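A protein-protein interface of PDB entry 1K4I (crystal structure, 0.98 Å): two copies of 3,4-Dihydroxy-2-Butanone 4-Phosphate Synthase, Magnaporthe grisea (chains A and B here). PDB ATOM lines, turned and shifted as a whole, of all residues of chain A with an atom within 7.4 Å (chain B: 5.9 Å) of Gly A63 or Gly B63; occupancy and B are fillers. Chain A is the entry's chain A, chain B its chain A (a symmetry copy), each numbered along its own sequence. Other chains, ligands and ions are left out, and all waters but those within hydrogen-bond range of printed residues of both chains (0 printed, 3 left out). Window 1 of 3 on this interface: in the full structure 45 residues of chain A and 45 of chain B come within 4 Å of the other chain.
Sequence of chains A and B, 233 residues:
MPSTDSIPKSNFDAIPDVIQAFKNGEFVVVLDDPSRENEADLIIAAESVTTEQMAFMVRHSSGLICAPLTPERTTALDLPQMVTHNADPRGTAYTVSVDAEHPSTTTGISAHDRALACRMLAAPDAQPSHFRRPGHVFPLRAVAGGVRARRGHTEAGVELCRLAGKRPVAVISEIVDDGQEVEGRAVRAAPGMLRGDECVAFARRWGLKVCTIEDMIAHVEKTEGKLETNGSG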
ATOM      1  N   MET A  57     -18.781 -14.876  31.630  1.00  0.00           N
ATOM      2  CA  MET A  57     -20.230 -14.895  31.701  1.00  0.00           C
ATOM      3  C   MET A  57     -20.779 -16.299  31.486  1.00  0.00           C
ATOM      4  O   MET A  57     -21.681 -16.761  32.228  1.00  0.00           O
ATOM      5  CB  MET A  57     -20.820 -13.938  30.649  1.00  0.00           C
ATOM      6  CG  MET A  57     -22.284 -13.611  30.892  1.00  0.00           C
ATOM      7  SD  MET A  57     -22.846 -12.418  29.643  1.00  0.00           S
ATOM      8  CE  MET A  57     -24.158 -11.601  30.582  1.00  0.00           C
ATOM      9  N   VAL A  58     -20.242 -16.997  30.494  1.00  0.00           N
ATOM     10  CA  VAL A  58     -20.703 -18.358  30.229  1.00  0.00           C
ATOM     11  C   VAL A  58     -20.385 -19.262  31.412  1.00  0.00           C
ATOM     12  O   VAL A  58     -21.217 -20.088  31.833  1.00  0.00           O
ATOM     13  CB  VAL A  58     -20.097 -18.858  28.927  1.00  0.00           C
ATOM     14  CG1 VAL A  58     -20.388 -20.343  28.718  1.00  0.00           C
ATOM     15  CG2 VAL A  58     -20.711 -18.087  27.742  1.00  0.00           C
ATOM     16  N   ARG A  59     -19.190 -19.135  31.955  1.00  0.00           N
ATOM     17  CA  ARG A  59     -18.790 -19.996  33.057  1.00  0.00           C
ATOM     18  C   ARG A  59     -19.675 -19.855  34.270  1.00  0.00           C
ATOM     19  O   ARG A  59     -19.946 -20.864  34.950  1.00  0.00           O
ATOM     20  CB  ARG A  59     -17.341 -19.703  33.423  1.00  0.00           C
ATOM     21  CG  ARG A  59     -16.915 -20.259  34.792  1.00  0.00           C
ATOM     22  CD  ARG A  59     -16.834 -21.799  34.771  1.00  0.00           C
ATOM     23  NE  ARG A  59     -16.291 -22.259  36.046  1.00  0.00           N
ATOM     24  CZ  ARG A  59     -17.039 -22.228  37.148  1.00  0.00           C
ATOM     25  NH1 ARG A  59     -18.343 -21.884  37.144  1.00  0.00           N
ATOM     26  NH2 ARG A  59     -16.455 -22.619  38.287  1.00  0.00           N
ATOM     27  N   HIS A  60     -20.086 -18.625  34.598  1.00  0.00           N
ATOM     28  CA  HIS A  60     -20.822 -18.398  35.827  1.00  0.00           C
ATOM     29  C   HIS A  60     -22.320 -18.267  35.677  1.00  0.00           C
ATOM     30  O   HIS A  60     -23.038 -18.129  36.676  1.00  0.00           O
ATOM     31  CB  HIS A  60     -20.246 -17.155  36.565  1.00  0.00           C
ATOM     32  CG  HIS A  60     -18.847 -17.397  37.006  1.00  0.00           C
ATOM     33  ND1 HIS A  60     -18.555 -18.181  38.107  1.00  0.00           N
ATOM     34  CD2 HIS A  60     -17.669 -16.992  36.445  1.00  0.00           C
ATOM     35  CE1 HIS A  60     -17.216 -18.224  38.200  1.00  0.00           C
ATOM     36  NE2 HIS A  60     -16.648 -17.530  37.221  1.00  0.00           N
ATOM     37  N   SER A  61     -22.829 -18.348  34.459  1.00  0.00           N
ATOM     38  CA  SER A  61     -24.255 -18.200  34.268  1.00  0.00           C
ATOM     39  C   SER A  61     -24.868 -19.489  33.728  1.00  0.00           C
ATOM     40  O   SER A  61     -24.220 -20.502  33.554  1.00  0.00           O
ATOM     41  CB  SER A  61     -24.517 -17.054  33.305  1.00  0.00           C
ATOM     42  OG  SER A  61     -24.211 -17.440  31.982  1.00  0.00           O
ATOM     43  N   SER A  62     -26.172 -19.390  33.428  1.00  0.00           N
ATOM     44  CA  SER A  62     -26.888 -20.501  32.811  1.00  0.00           C
ATOM     45  C   SER A  62     -26.292 -20.823  31.431  1.00  0.00           C
ATOM     46  O   SER A  62     -26.546 -21.915  30.879  1.00  0.00           O
ATOM     47  CB  SER A  62     -28.350 -20.102  32.641  1.00  0.00           C
ATOM     48  OG  SER A  62     -28.435 -19.079  31.645  1.00  0.00           O
ATOM     49  N   GLY A  63     -25.570 -19.860  30.834  1.00  0.00           N
ATOM     50  CA  GLY A  63     -25.063 -20.065  29.478  1.00  0.00           C
ATOM     51  C   GLY A  63     -26.065 -19.673  28.397  1.00  0.00           C
ATOM     52  O   GLY A  63     -25.730 -19.698  27.208  1.00  0.00           O
ATOM     53  N   LEU A  64     -27.309 -19.319  28.770  1.00  0.00           N
ATOM     54  CA  LEU A  64     -28.258 -18.854  27.786  1.00  0.00           C
ATOM     55  C   LEU A  64     -28.043 -17.343  27.762  1.00  0.00           C
ATOM     56  O   LEU A  64     -28.563 -16.582  28.600  1.00  0.00           O
ATOM     57  CB  LEU A  64     -29.666 -19.307  28.193  1.00  0.00           C
ATOM     58  CG  LEU A  64     -30.809 -18.912  27.292  1.00  0.00           C
ATOM     59  CD1 LEU A  64     -30.357 -18.969  25.840  1.00  0.00           C
ATOM     60  CD2 LEU A  64     -31.947 -19.906  27.585  1.00  0.00           C
ATOM     61  N   ILE A  65     -27.138 -16.925  26.868  1.00  0.00           N
ATOM     62  CA  ILE A  65     -26.695 -15.539  26.767  1.00  0.00           C
ATOM     63  C   ILE A  65     -27.670 -14.784  25.883  1.00  0.00           C
ATOM     64  O   ILE A  65     -27.824 -15.110  24.703  1.00  0.00           O
ATOM     65  CB  ILE A  65     -25.254 -15.474  26.213  1.00  0.00           C
ATOM     66  CG1 ILE A  65     -24.249 -16.338  26.988  1.00  0.00           C
ATOM     67  CG2 ILE A  65     -24.814 -14.012  26.145  1.00  0.00           C
ATOM     68  CD1 ILE A  65     -24.220 -15.999  28.472  1.00  0.00           C
ATOM     69  N   CYS A  66     -28.326 -13.782  26.464  1.00  0.00           N
ATOM     70  CA  CYS A  66     -29.334 -12.991  25.786  1.00  0.00           C
ATOM     71  C   CYS A  66     -28.850 -11.556  25.607  1.00  0.00           C
ATOM     72  O   CYS A  66     -27.960 -11.098  26.323  1.00  0.00           O
ATOM     73  CB  CYS A  66     -30.632 -12.992  26.608  1.00  0.00           C
ATOM     74  SG  CYS A  66     -31.332 -14.656  26.810  1.00  0.00           S
ATOM     75  N   ILE A 109     -20.964 -20.641  18.747  1.00  0.00           N
ATOM     76  CA  ILE A 109     -21.148 -20.852  20.188  1.00  0.00           C
ATOM     77  C   ILE A 109     -19.998 -20.418  21.095  1.00  0.00           C
ATOM     78  O   ILE A 109     -20.205 -20.210  22.289  1.00  0.00           O
ATOM     79  CB  ILE A 109     -21.449 -22.357  20.415  1.00  0.00           C
ATOM     80  CG1 ILE A 109     -22.005 -22.644  21.818  1.00  0.00           C
ATOM     81  CG2 ILE A 109     -20.199 -23.210  20.205  1.00  0.00           C
ATOM     82  CD1 ILE A 109     -23.357 -21.970  22.065  1.00  0.00           C
ATOM     83  N   ARG A 114     -19.891 -15.537  20.422  1.00  0.00           N
ATOM     84  CA  ARG A 114     -21.058 -14.931  21.080  1.00  0.00           C
ATOM     85  C   ARG A 114     -20.771 -13.470  21.422  1.00  0.00           C
ATOM     86  O   ARG A 114     -21.652 -12.613  21.256  1.00  0.00           O
ATOM     87  CB  ARG A 114     -21.562 -15.766  22.261  1.00  0.00           C
ATOM     88  CG  ARG A 114     -22.225 -17.057  21.748  1.00  0.00           C
ATOM     89  CD  ARG A 114     -23.095 -17.743  22.826  1.00  0.00           C
ATOM     90  NE  ARG A 114     -22.325 -18.631  23.698  1.00  0.00           N
ATOM     91  CZ  ARG A 114     -22.909 -19.329  24.689  1.00  0.00           C
ATOM     92  NH1 ARG A 114     -24.206 -19.172  24.975  1.00  0.00           N
ATOM     93  NH2 ARG A 114     -22.160 -20.154  25.407  1.00  0.00           N
ATOM     94  N   HIS A 136     -26.969 -18.557  17.989  1.00  0.00           N
ATOM     95  CA  HIS A 136     -26.689 -18.912  19.366  1.00  0.00           C
ATOM     96  C   HIS A 136     -26.745 -17.798  20.379  1.00  0.00           C
ATOM     97  O   HIS A 136     -26.447 -18.044  21.538  1.00  0.00           O
ATOM     98  CB  HIS A 136     -25.323 -19.629  19.457  1.00  0.00           C
ATOM     99  CG  HIS A 136     -25.173 -20.776  18.501  1.00  0.00           C
ATOM    100  ND1 HIS A 136     -24.924 -20.588  17.138  1.00  0.00           N
ATOM    101  CD2 HIS A 136     -25.246 -22.119  18.712  1.00  0.00           C
ATOM    102  CE1 HIS A 136     -24.885 -21.788  16.546  1.00  0.00           C
ATOM    103  NE2 HIS A 136     -25.058 -22.727  17.484  1.00  0.00           N
ATOM    104  N   PHE A 138     -29.416 -14.745  21.883  1.00  0.00           N
ATOM    105  CA  PHE A 138     -30.864 -14.531  21.956  1.00  0.00           C
ATOM    106  C   PHE A 138     -31.246 -13.103  22.288  1.00  0.00           C
ATOM    107  O   PHE A 138     -31.305 -12.715  23.455  1.00  0.00           O
ATOM    108  CB  PHE A 138     -31.414 -15.508  23.035  1.00  0.00           C
ATOM    109  CG  PHE A 138     -31.186 -16.921  22.563  1.00  0.00           C
ATOM    110  CD1 PHE A 138     -29.998 -17.577  22.873  1.00  0.00           C
ATOM    111  CD2 PHE A 138     -32.124 -17.549  21.755  1.00  0.00           C
ATOM    112  CE1 PHE A 138     -29.767 -18.862  22.373  1.00  0.00           C
ATOM    113  CE2 PHE A 138     -31.905 -18.822  21.232  1.00  0.00           C
ATOM    114  CZ  PHE A 138     -30.710 -19.462  21.548  1.00  0.00           C
ATOM    115  N   ILE A 172     -27.322 -10.193  28.943  1.00  0.00           N
ATOM    116  CA  ILE A 172     -27.732 -10.691  30.245  1.00  0.00           C
ATOM    117  C   ILE A 172     -27.753 -12.205  30.269  1.00  0.00           C
ATOM    118  O   ILE A 172     -27.973 -12.858  29.250  1.00  0.00           O
ATOM    119  CB  ILE A 172     -29.105 -10.186  30.706  1.00  0.00           C
ATOM    120  CG1 ILE A 172     -30.276 -10.765  29.891  1.00  0.00           C
ATOM    121  CG2 ILE A 172     -29.133  -8.651  30.688  1.00  0.00           C
ATOM    122  CD1 ILE A 172     -31.679 -10.375  30.421  1.00  0.00           C
ATOM    123  N   SER A 173     -27.563 -12.744  31.482  1.00  0.00           N
ATOM    124  CA  SER A 173     -27.734 -14.176  31.707  1.00  0.00           C
ATOM    125  C   SER A 173     -27.919 -14.390  33.201  1.00  0.00           C
ATOM    126  O   SER A 173     -27.368 -13.620  34.006  1.00  0.00           O
ATOM    127  CB  SER A 173     -26.565 -14.987  31.155  1.00  0.00           C
ATOM    128  OG  SER A 173     -26.946 -16.367  31.133  1.00  0.00           O
ATOM    129  N   GLU A 174     -28.664 -15.428  33.577  1.00  0.00           N
ATOM    130  CA  GLU A 174     -28.920 -15.699  34.989  1.00  0.00           C
ATOM    131  C   GLU A 174     -27.725 -16.344  35.699  1.00  0.00           C
ATOM    132  O   GLU A 174     -27.079 -17.248  35.152  1.00  0.00           O
ATOM    133  CB  GLU A 174     -30.069 -16.684  35.158  1.00  0.00           C
ATOM    134  CG  GLU A 174     -31.356 -16.284  34.418  1.00  0.00           C
ATOM    135  CD  GLU A 174     -31.425 -16.857  33.024  1.00  0.00           C
ATOM    136  OE1 GLU A 174     -30.412 -17.133  32.370  1.00  0.00           O
ATOM    137  OE2 GLU A 174     -32.671 -17.074  32.614  1.00  0.00           O
ATOM    138  N   VAL A 176     -26.393 -18.907  38.004  1.00  0.00           N
ATOM    139  CA  VAL A 176     -26.877 -20.161  38.603  1.00  0.00           C
ATOM    140  C   VAL A 176     -26.013 -20.547  39.802  1.00  0.00           C
ATOM    141  O   VAL A 176     -24.939 -20.016  40.047  1.00  0.00           O
ATOM    142  CB  VAL A 176     -26.811 -21.296  37.564  1.00  0.00           C
ATOM    143  CG1 VAL A 176     -27.684 -20.990  36.345  1.00  0.00           C
ATOM    144  CG2 VAL A 176     -25.368 -21.609  37.163  1.00  0.00           C
ATOM    145  N   MET B  57     -23.983 -30.785  33.184  1.00  0.00           N
ATOM    146  CA  MET B  57     -23.976 -30.425  31.779  1.00  0.00           C
ATOM    147  C   MET B  57     -23.863 -28.918  31.592  1.00  0.00           C
ATOM    148  O   MET B  57     -23.071 -28.429  30.748  1.00  0.00           O
ATOM    149  CB  MET B  57     -25.258 -30.939  31.099  1.00  0.00           C
ATOM    150  CG  MET B  57     -25.171 -30.940  29.582  1.00  0.00           C
ATOM    151  SD  MET B  57     -26.701 -31.639  28.895  1.00  0.00           S
ATOM    152  CE  MET B  57     -26.054 -32.298  27.340  1.00  0.00           C
ATOM    153  N   VAL B  58     -24.625 -28.166  32.375  1.00  0.00           N
ATOM    154  CA  VAL B  58     -24.566 -26.710  32.268  1.00  0.00           C
ATOM    155  C   VAL B  58     -23.183 -26.208  32.659  1.00  0.00           C
ATOM    156  O   VAL B  58     -22.609 -25.321  31.999  1.00  0.00           O
ATOM    157  CB  VAL B  58     -25.674 -26.091  33.106  1.00  0.00           C
ATOM    158  CG1 VAL B  58     -25.522 -24.574  33.185  1.00  0.00           C
ATOM    159  CG2 VAL B  58     -27.040 -26.394  32.458  1.00  0.00           C
ATOM    160  N   SER B  61     -20.572 -27.162  29.767  1.00  0.00           N
ATOM    161  CA  SER B  61     -20.859 -26.905  28.373  1.00  0.00           C
ATOM    162  C   SER B  61     -21.090 -25.417  28.131  1.00  0.00           C
ATOM    163  O   SER B  61     -20.979 -24.583  29.008  1.00  0.00           O
ATOM    164  CB  SER B  61     -22.086 -27.699  27.958  1.00  0.00           C
ATOM    165  OG  SER B  61     -23.257 -27.108  28.480  1.00  0.00           O
ATOM    166  N   SER B  62     -21.465 -25.118  26.878  1.00  0.00           N
ATOM    167  CA  SER B  62     -21.821 -23.753  26.504  1.00  0.00           C
ATOM    168  C   SER B  62     -23.049 -23.282  27.298  1.00  0.00           C
ATOM    169  O   SER B  62     -23.325 -22.064  27.359  1.00  0.00           O
ATOM    170  CB  SER B  62     -22.151 -23.729  25.015  1.00  0.00           C
ATOM    171  OG  SER B  62     -23.372 -24.442  24.803  1.00  0.00           O
ATOM    172  N   GLY B  63     -23.832 -24.231  27.839  1.00  0.00           N
ATOM    173  CA  GLY B  63     -25.070 -23.852  28.518  1.00  0.00           C
ATOM    174  C   GLY B  63     -26.259 -23.726  27.571  1.00  0.00           C
ATOM    175  O   GLY B  63     -27.388 -23.513  28.025  1.00  0.00           O
ATOM    176  N   LEU B  64     -26.043 -23.837  26.247  1.00  0.00           N
ATOM    177  CA  LEU B  64     -27.155 -23.815  25.325  1.00  0.00           C
ATOM    178  C   LEU B  64     -27.541 -25.285  25.189  1.00  0.00           C
ATOM    179  O   LEU B  64     -26.943 -26.064  24.424  1.00  0.00           O
ATOM    180  CB  LEU B  64     -26.712 -23.133  24.024  1.00  0.00           C
ATOM    181  CG  LEU B  64     -27.735 -23.016  22.921  1.00  0.00           C
ATOM    182  CD1 LEU B  64     -29.105 -22.742  23.523  1.00  0.00           C
ATOM    183  CD2 LEU B  64     -27.258 -21.866  22.017  1.00  0.00           C
ATOM    184  N   ILE B  65     -28.468 -25.698  26.063  1.00  0.00           N
ATOM    185  CA  ILE B  65     -28.889 -27.090  26.185  1.00  0.00           C
ATOM    186  C   ILE B  65     -29.975 -27.356  25.161  1.00  0.00           C
ATOM    187  O   ILE B  65     -31.045 -26.741  25.210  1.00  0.00           O
ATOM    188  CB  ILE B  65     -29.375 -27.380  27.623  1.00  0.00           C
ATOM    189  CG1 ILE B  65     -28.365 -26.993  28.712  1.00  0.00           C
ATOM    190  CG2 ILE B  65     -29.782 -28.850  27.721  1.00  0.00           C
ATOM    191  CD1 ILE B  65     -27.011 -27.659  28.508  1.00  0.00           C
ATOM    192  N   ARG B 114     -34.717 -27.322  33.433  1.00  0.00           N
ATOM    193  CA  ARG B 114     -34.285 -27.754  32.096  1.00  0.00           C
ATOM    194  C   ARG B 114     -34.302 -29.279  32.003  1.00  0.00           C
ATOM    195  O   ARG B 114     -34.715 -29.830  30.971  1.00  0.00           O
ATOM    196  CB  ARG B 114     -32.958 -27.114  31.676  1.00  0.00           C
ATOM    197  CG  ARG B 114     -33.166 -25.617  31.383  1.00  0.00           C
ATOM    198  CD  ARG B 114     -31.993 -25.002  30.585  1.00  0.00           C
ATOM    199  NE  ARG B 114     -30.894 -24.557  31.443  1.00  0.00           N
ATOM    200  CZ  ARG B 114     -29.789 -23.982  30.934  1.00  0.00           C
ATOM    201  NH1 ARG B 114     -29.610 -23.874  29.612  1.00  0.00           N
ATOM    202  NH2 ARG B 114     -28.856 -23.555  31.773  1.00  0.00           N
ATOM    203  N   SER B 173     -25.057 -30.586  24.213  1.00  0.00           N
ATOM    204  CA  SER B 173     -24.493 -29.247  24.351  1.00  0.00           C
ATOM    205  C   SER B 173     -23.002 -29.341  24.066  1.00  0.00           C
ATOM    206  O   SER B 173     -22.388 -30.387  24.339  1.00  0.00           O
ATOM    207  CB  SER B 173     -24.773 -28.646  25.726  1.00  0.00           C
ATOM    208  OG  SER B 173     -24.470 -27.247  25.676  1.00  0.00           O
ATOM    209  N   GLU B 174     -22.416 -28.266  23.543  1.00  0.00           N
ATOM    210  CA  GLU B 174     -20.994 -28.270  23.209  1.00  0.00           C
ATOM    211  C   GLU B 174     -20.092 -28.121  24.440  1.00  0.00           C
ATOM    212  O   GLU B 174     -20.368 -27.305  25.329  1.00  0.00           O
ATOM    213  CB  GLU B 174     -20.640 -27.097  22.306  1.00  0.00           C
ATOM    214  CG  GLU B 174     -21.513 -26.987  21.046  1.00  0.00           C
ATOM    215  CD  GLU B 174     -22.724 -26.111  21.255  1.00  0.00           C
ATOM    216  OE1 GLU B 174     -23.243 -25.952  22.367  1.00  0.00           O
ATOM    217  OE2 GLU B 174     -23.125 -25.505  20.142  1.00  0.00           O
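The guanidinium group (NH2) of Arg A114 sits at hydrogen-bond distance from the backbone carbonyl oxygen (O) of Ser B62, 3.0 Å away. O of Gly A63 lies close to O of Ser B62 (3.4 Å). O of Gly B63 sits close to O of Ser A62 (3.4 Å). The backbone carbonyl oxygen (O) of Ser A62 lies within hydrogen-bond range of the guanidinium group (NH2) of Arg B114, 3.0 Å away.
The backbone NH of Phe A138 sits at hydrogen-bond distance from the backbone carbonyl oxygen of Ile A65. The side-chain hydroxyl of Ser B62 sits at hydrogen-bond distance from the side-chain hydroxyl of Ser B173, at 3.1 Å. O of Gly A63 sits at hydrogen-bond distance from NH1 of Arg A114 (2.8 Å). The guanidinium group (NE) of Arg A114 is in hydrogen-bond range of the backbone carbonyl oxygen (O) of Ile A109, at 3.0 Å. O of Leu B64 sits at hydrogen-bond distance from OG of Ser B173 (3.0 Å). The backbone NH (N) of Leu A64 lies within hydrogen-bond range of the side-chain hydroxyl (OG) of Ser A62 (3.1 Å).
O of Ser B62 touches CG1 of Val A58 (3.7 Å). Val B58 touches Ser A62. Gly B63 touches Gly A63 (CA to CA, 3.9 Å). Ser B62 touches Ile A109. CD1 of Ile A109 touches CD2 of Leu B64 (3.9 Å). CG1 of Ile A109 touches OE2 of Glu B174 (3.5 Å). His A136 touches Leu B64 (CD2 to CD2, 3.9 Å). Leu B64 touches Phe A138.
Ser A61 touches none of the printed residues of chain B. Of chain B, only Ser B62 (3.4 Å) and Gly B63 (3.9 Å) come within 4 Å of Gly A63. Printed residues of chain B within 4 Å of Ile A109: Ser B62, Leu B64 and Glu B174. Of the printed residues of chain B, His A136 touches Leu B64. Of the printed residues of chain B, Phe A138 touches Leu B64 (3.9 Å). Val A176 touches none of the printed residues of chain B. Of the printed residues of chain A, Val B58 touches Ser A62 (3.7 Å). Gly B63 touches just these residues of chain A: Ser A62 and Gly A63. Printed residues of chain A within 4 Å of Glu B174: Ile A109. The nearest residue of chain B that does not touch Gly A63 is Leu B64 (4.3 Å).
Of the 10 printed residues of chain B, 6 touch a printed residue of chain A. Of the 18 printed residues of chain A, 7 touch a printed residue of chain B. Among the printed residues, no Asp or Glu carboxylate lies within 4 Å of a Lys or Arg side-chain nitrogen of the other chain.
Val A58 touches Ser B62, and with the chains exchanged Ser A62 touches Val B58. Ser A62 touches Gly B63, and with the chains exchanged Gly A63 touches Ser B62. Ser A62 touches Arg B114, and with the chains exchanged Arg A114 touches Ser B62. Gly B63 touches its own counterpart, Gly A63. Positions printed for both chains: 57, 58, 61, 62, 63, 64, 65, 114, 173 and 174.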
